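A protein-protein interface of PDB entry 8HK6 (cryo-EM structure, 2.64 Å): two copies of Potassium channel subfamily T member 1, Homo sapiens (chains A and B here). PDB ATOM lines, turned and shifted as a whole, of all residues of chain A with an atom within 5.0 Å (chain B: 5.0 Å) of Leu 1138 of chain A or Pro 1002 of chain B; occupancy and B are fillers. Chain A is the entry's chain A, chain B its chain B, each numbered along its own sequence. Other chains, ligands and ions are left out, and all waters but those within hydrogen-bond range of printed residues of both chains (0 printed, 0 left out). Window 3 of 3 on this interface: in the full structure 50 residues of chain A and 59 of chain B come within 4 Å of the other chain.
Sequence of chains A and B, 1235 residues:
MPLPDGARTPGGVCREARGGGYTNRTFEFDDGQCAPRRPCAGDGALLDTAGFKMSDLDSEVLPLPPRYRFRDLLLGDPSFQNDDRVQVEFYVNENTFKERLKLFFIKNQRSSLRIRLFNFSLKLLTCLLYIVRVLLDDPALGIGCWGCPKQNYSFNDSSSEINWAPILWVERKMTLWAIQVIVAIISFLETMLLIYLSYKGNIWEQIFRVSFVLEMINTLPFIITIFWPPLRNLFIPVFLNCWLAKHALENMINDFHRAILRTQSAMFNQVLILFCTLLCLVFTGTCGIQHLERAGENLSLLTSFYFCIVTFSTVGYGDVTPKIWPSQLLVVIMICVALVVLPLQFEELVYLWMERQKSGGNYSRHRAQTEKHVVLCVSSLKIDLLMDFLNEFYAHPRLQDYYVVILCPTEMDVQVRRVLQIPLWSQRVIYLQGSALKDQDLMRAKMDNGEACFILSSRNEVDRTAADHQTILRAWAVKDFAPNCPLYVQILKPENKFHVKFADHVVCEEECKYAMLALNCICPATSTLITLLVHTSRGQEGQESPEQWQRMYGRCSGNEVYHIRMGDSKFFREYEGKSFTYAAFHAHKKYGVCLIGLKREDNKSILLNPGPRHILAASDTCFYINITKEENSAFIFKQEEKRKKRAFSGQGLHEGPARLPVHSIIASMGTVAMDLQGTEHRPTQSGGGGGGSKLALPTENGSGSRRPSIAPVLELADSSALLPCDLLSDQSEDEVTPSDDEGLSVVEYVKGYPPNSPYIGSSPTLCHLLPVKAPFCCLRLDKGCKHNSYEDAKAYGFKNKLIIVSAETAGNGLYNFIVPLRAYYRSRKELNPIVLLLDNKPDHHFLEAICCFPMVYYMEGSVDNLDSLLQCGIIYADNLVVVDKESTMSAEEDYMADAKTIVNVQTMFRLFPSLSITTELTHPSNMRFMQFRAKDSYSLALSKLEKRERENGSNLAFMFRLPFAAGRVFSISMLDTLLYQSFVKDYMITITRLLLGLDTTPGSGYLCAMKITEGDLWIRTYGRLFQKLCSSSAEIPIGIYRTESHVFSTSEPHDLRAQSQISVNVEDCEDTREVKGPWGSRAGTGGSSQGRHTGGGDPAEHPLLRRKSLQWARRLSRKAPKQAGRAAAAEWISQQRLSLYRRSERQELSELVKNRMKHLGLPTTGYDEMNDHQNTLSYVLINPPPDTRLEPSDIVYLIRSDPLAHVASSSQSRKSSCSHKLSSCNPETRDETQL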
ATOM      1  N   SER A1134      19.646 -20.735 -23.584  1.00  0.00           N
ATOM      2  CA  SER A1134      19.975 -22.146 -23.412  1.00  0.00           C
ATOM      3  C   SER A1134      21.404 -22.324 -22.914  1.00  0.00           C
ATOM      4  O   SER A1134      21.684 -23.243 -22.135  1.00  0.00           O
ATOM      5  CB  SER A1134      19.767 -22.898 -24.725  1.00  0.00           C
ATOM      6  OG  SER A1134      18.398 -22.910 -25.094  1.00  0.00           O
ATOM      7  N   GLN A1135      22.320 -21.462 -23.357  1.00  0.00           N
ATOM      8  CA  GLN A1135      23.712 -21.571 -22.929  1.00  0.00           C
ATOM      9  C   GLN A1135      23.846 -21.341 -21.429  1.00  0.00           C
ATOM     10  O   GLN A1135      24.482 -22.131 -20.722  1.00  0.00           O
ATOM     11  CB  GLN A1135      24.576 -20.580 -23.707  1.00  0.00           C
ATOM     12  N   GLN A1136      23.247 -20.261 -20.923  1.00  0.00           N
ATOM     13  CA  GLN A1136      23.299 -20.006 -19.489  1.00  0.00           C
ATOM     14  C   GLN A1136      22.505 -21.047 -18.711  1.00  0.00           C
ATOM     15  O   GLN A1136      22.896 -21.422 -17.601  1.00  0.00           O
ATOM     16  CB  GLN A1136      22.794 -18.594 -19.186  1.00  0.00           C
ATOM     17  CG  GLN A1136      21.417 -18.283 -19.748  1.00  0.00           C
ATOM     18  CD  GLN A1136      21.212 -16.805 -20.018  1.00  0.00           C
ATOM     19  OE1 GLN A1136      20.133 -16.262 -19.785  1.00  0.00           O
ATOM     20  NE2 GLN A1136      22.251 -16.146 -20.519  1.00  0.00           N
ATOM     21  N   ARG A1137      21.410 -21.546 -19.289  1.00  0.00           N
ATOM     22  CA  ARG A1137      20.581 -22.531 -18.600  1.00  0.00           C
ATOM     23  C   ARG A1137      21.361 -23.807 -18.310  1.00  0.00           C
ATOM     24  O   ARG A1137      21.261 -24.373 -17.215  1.00  0.00           O
ATOM     25  CB  ARG A1137      19.340 -22.842 -19.434  1.00  0.00           C
ATOM     26  CG  ARG A1137      18.405 -21.667 -19.601  1.00  0.00           C
ATOM     27  CD  ARG A1137      17.248 -22.012 -20.516  1.00  0.00           C
ATOM     28  NE  ARG A1137      16.414 -23.061 -19.944  1.00  0.00           N
ATOM     29  CZ  ARG A1137      15.402 -23.642 -20.572  1.00  0.00           C
ATOM     30  NH1 ARG A1137      15.045 -23.280 -21.793  1.00  0.00           N
ATOM     31  NH2 ARG A1137      14.731 -24.612 -19.961  1.00  0.00           N
ATOM     32  N   LEU A1138      22.135 -24.284 -19.285  1.00  0.00           N
ATOM     33  CA  LEU A1138      22.967 -25.458 -19.050  1.00  0.00           C
ATOM     34  C   LEU A1138      24.080 -25.146 -18.060  1.00  0.00           C
ATOM     35  O   LEU A1138      24.447 -25.995 -17.240  1.00  0.00           O
ATOM     36  CB  LEU A1138      23.544 -25.967 -20.370  1.00  0.00           C
ATOM     37  CG  LEU A1138      23.597 -27.487 -20.537  1.00  0.00           C
ATOM     38  CD1 LEU A1138      22.300 -28.128 -20.066  1.00  0.00           C
ATOM     39  CD2 LEU A1138      23.889 -27.862 -21.982  1.00  0.00           C
ATOM     40  N   SER A1139      24.627 -23.930 -18.121  1.00  0.00           N
ATOM     41  CA  SER A1139      25.697 -23.543 -17.209  1.00  0.00           C
ATOM     42  C   SER A1139      25.218 -23.536 -15.761  1.00  0.00           C
ATOM     43  O   SER A1139      25.903 -24.045 -14.868  1.00  0.00           O
ATOM     44  CB  SER A1139      26.243 -22.170 -17.601  1.00  0.00           C
ATOM     45  OG  SER A1139      27.130 -21.674 -16.617  1.00  0.00           O
ATOM     46  N   LEU A1140      24.039 -22.962 -15.509  1.00  0.00           N
ATOM     47  CA  LEU A1140      23.525 -22.930 -14.143  1.00  0.00           C
ATOM     48  C   LEU A1140      23.124 -24.314 -13.657  1.00  0.00           C
ATOM     49  O   LEU A1140      23.091 -24.558 -12.446  1.00  0.00           O
ATOM     50  CB  LEU A1140      22.340 -21.970 -14.034  1.00  0.00           C
ATOM     51  CG  LEU A1140      22.611 -20.490 -14.301  1.00  0.00           C
ATOM     52  CD1 LEU A1140      21.569 -19.906 -15.229  1.00  0.00           C
ATOM     53  CD2 LEU A1140      22.653 -19.715 -12.997  1.00  0.00           C
ATOM     54  N   TYR A1141      22.801 -25.224 -14.572  1.00  0.00           N
ATOM     55  CA  TYR A1141      22.471 -26.584 -14.170  1.00  0.00           C
ATOM     56  C   TYR A1141      23.720 -27.388 -13.835  1.00  0.00           C
ATOM     57  O   TYR A1141      23.699 -28.224 -12.926  1.00  0.00           O
ATOM     58  CB  TYR A1141      21.666 -27.275 -15.269  1.00  0.00           C
ATOM     59  CG  TYR A1141      21.145 -28.633 -14.875  1.00  0.00           C
ATOM     60  CD1 TYR A1141      21.636 -29.785 -15.470  1.00  0.00           C
ATOM     61  CD2 TYR A1141      20.168 -28.765 -13.900  1.00  0.00           C
ATOM     62  CE1 TYR A1141      21.166 -31.027 -15.111  1.00  0.00           C
ATOM     63  CE2 TYR A1141      19.690 -30.003 -13.534  1.00  0.00           C
ATOM     64  CZ  TYR A1141      20.193 -31.132 -14.144  1.00  0.00           C
ATOM     65  OH  TYR A1141      19.722 -32.372 -13.782  1.00  0.00           O
ATOM     66  N   ARG A1142      24.815 -27.153 -14.558  1.00  0.00           N
ATOM     67  CA  ARG A1142      26.050 -27.891 -14.335  1.00  0.00           C
ATOM     68  C   ARG A1142      26.868 -27.354 -13.169  1.00  0.00           C
ATOM     69  O   ARG A1142      27.793 -28.039 -12.721  1.00  0.00           O
ATOM     70  CB  ARG A1142      26.915 -27.874 -15.598  1.00  0.00           C
ATOM     71  CG  ARG A1142      26.288 -28.539 -16.809  1.00  0.00           C
ATOM     72  CD  ARG A1142      26.545 -30.033 -16.818  1.00  0.00           C
ATOM     73  NE  ARG A1142      25.557 -30.749 -16.021  1.00  0.00           N
ATOM     74  CZ  ARG A1142      25.806 -31.315 -14.848  1.00  0.00           C
ATOM     75  NH1 ARG A1142      27.012 -31.274 -14.304  1.00  0.00           N
ATOM     76  NH2 ARG A1142      24.822 -31.932 -14.202  1.00  0.00           N
ATOM     77  N   LEU B 607      12.939 -36.598 -16.942  1.00  0.00           N
ATOM     78  CA  LEU B 607      12.366 -35.552 -17.776  1.00  0.00           C
ATOM     79  C   LEU B 607      10.870 -35.770 -17.922  1.00  0.00           C
ATOM     80  O   LEU B 607      10.437 -36.843 -18.347  1.00  0.00           O
ATOM     81  CB  LEU B 607      13.028 -35.527 -19.154  1.00  0.00           C
ATOM     82  CG  LEU B 607      14.534 -35.282 -19.157  1.00  0.00           C
ATOM     83  CD1 LEU B 607      15.050 -35.156 -20.575  1.00  0.00           C
ATOM     84  CD2 LEU B 607      14.871 -34.046 -18.351  1.00  0.00           C
ATOM     85  N   THR B1000      14.525 -27.717 -11.840  1.00  0.00           N
ATOM     86  CA  THR B1000      14.456 -27.380 -13.258  1.00  0.00           C
ATOM     87  C   THR B1000      15.566 -28.128 -13.985  1.00  0.00           C
ATOM     88  O   THR B1000      16.729 -27.718 -13.949  1.00  0.00           O
ATOM     89  CB  THR B1000      14.580 -25.874 -13.468  1.00  0.00           C
ATOM     90  OG1 THR B1000      15.957 -25.492 -13.384  1.00  0.00           O
ATOM     91  CG2 THR B1000      13.794 -25.121 -12.407  1.00  0.00           C
ATOM     92  N   THR B1001      15.208 -29.218 -14.637  1.00  0.00           N
ATOM     93  CA  THR B1001      16.145 -29.928 -15.494  1.00  0.00           C
ATOM     94  C   THR B1001      15.962 -29.477 -16.931  1.00  0.00           C
ATOM     95  O   THR B1001      14.819 -29.404 -17.402  1.00  0.00           O
ATOM     96  CB  THR B1001      15.930 -31.435 -15.400  1.00  0.00           C
ATOM     97  OG1 THR B1001      15.727 -31.803 -14.032  1.00  0.00           O
ATOM     98  CG2 THR B1001      17.137 -32.167 -15.941  1.00  0.00           C
ATOM     99  N   PRO B1002      17.030 -29.143 -17.647  1.00  0.00           N
ATOM    100  CA  PRO B1002      16.880 -28.801 -19.065  1.00  0.00           C
ATOM    101  C   PRO B1002      16.272 -29.962 -19.838  1.00  0.00           C
ATOM    102  O   PRO B1002      16.700 -31.111 -19.706  1.00  0.00           O
ATOM    103  CB  PRO B1002      18.315 -28.504 -19.513  1.00  0.00           C
ATOM    104  CG  PRO B1002      19.025 -28.133 -18.257  1.00  0.00           C
ATOM    105  CD  PRO B1002      18.419 -28.985 -17.189  1.00  0.00           C
ATOM    106  N   GLY B1003      15.269 -29.652 -20.650  1.00  0.00           N
ATOM    107  CA  GLY B1003      14.545 -30.658 -21.391  1.00  0.00           C
ATOM    108  C   GLY B1003      13.380 -31.294 -20.667  1.00  0.00           C
ATOM    109  O   GLY B1003      12.838 -32.287 -21.163  1.00  0.00           O
ATOM    110  N   SER B1004      12.978 -30.760 -19.520  1.00  0.00           N
ATOM    111  CA  SER B1004      11.873 -31.295 -18.740  1.00  0.00           C
ATOM    112  C   SER B1004      10.696 -30.332 -18.799  1.00  0.00           C
ATOM    113  O   SER B1004      10.872 -29.114 -18.701  1.00  0.00           O
ATOM    114  CB  SER B1004      12.294 -31.530 -17.289  1.00  0.00           C
ATOM    115  OG  SER B1004      11.229 -32.043 -16.518  1.00  0.00           O
ATOM    116  N   ASP B1202       9.408 -28.731 -22.713  1.00  0.00           N
ATOM    117  CA  ASP B1202      10.244 -27.552 -22.532  1.00  0.00           C
ATOM    118  C   ASP B1202      10.310 -26.743 -23.824  1.00  0.00           C
ATOM    119  O   ASP B1202      10.614 -27.304 -24.886  1.00  0.00           O
ATOM    120  CB  ASP B1202      11.649 -27.967 -22.104  1.00  0.00           C
ATOM    121  CG  ASP B1202      12.411 -26.840 -21.454  1.00  0.00           C
ATOM    122  OD1 ASP B1202      12.904 -25.955 -22.183  1.00  0.00           O
ATOM    123  OD2 ASP B1202      12.528 -26.839 -20.212  1.00  0.00           O
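The guanidinium group (NH2) of Arg 1137 of chain A is in salt-bridge range of the side-chain carboxylate (OD2) of Asp 1202 of chain B (3.1 Å).
Among the printed residues, pairs that only touch across the chains: Leu 1138 of chain A with Pro 1002 of chain B, Tyr 1141 of chain A with Thr 1000 of chain B, Tyr 1141 of chain A with Thr 1001 of chain B and Tyr 1141 of chain A with Pro 1002 of chain B.
Pro 1002 of chain B touches two residues of chain A.
Printed residues of chain A within 4 Å of Asp 1202 of chain B: Arg 1137 (3.1 Å).
Printed residues of chain A within 4 Å of Thr 1000 of chain B: Tyr 1141.
Of the printed residues of chain A, Thr 1001 of chain B touches Tyr 1141.
Printed residues of chain B within 4 Å of Arg 1137 of chain A: Asp 1202 (3.1 Å).
Gln 1136 of chain A touches none of the printed residues of chain B.
The nearest printed residue of chain B that does not touch Tyr 1141 of chain A is Leu 607 of chain B (6.9 Å).
Of the 9 printed residues of chain A, 3 touch a printed residue of chain B.
Hydrophobic or aromatic side chains of chain A that line the printed part of chain B: Leu 1138 and Tyr 1141.
Printed residues of chain B that touch a printed residue of chain A: Thr 1000, Thr 1001, Pro 1002 and Asp 1202.
Among the printed residues, 5 pairs touch across the chains.
Among the printed residues, Asp or Glu carboxylates within 4 Å of a Lys or Arg side-chain nitrogen of the other chain: Arg 1137 of chain A with Asp 1202 of chain B.
No position is printed for both chains.
Of the 5 pairs that touch across the chains among the printed residues, none has its exchanged pair printed and touching as well.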
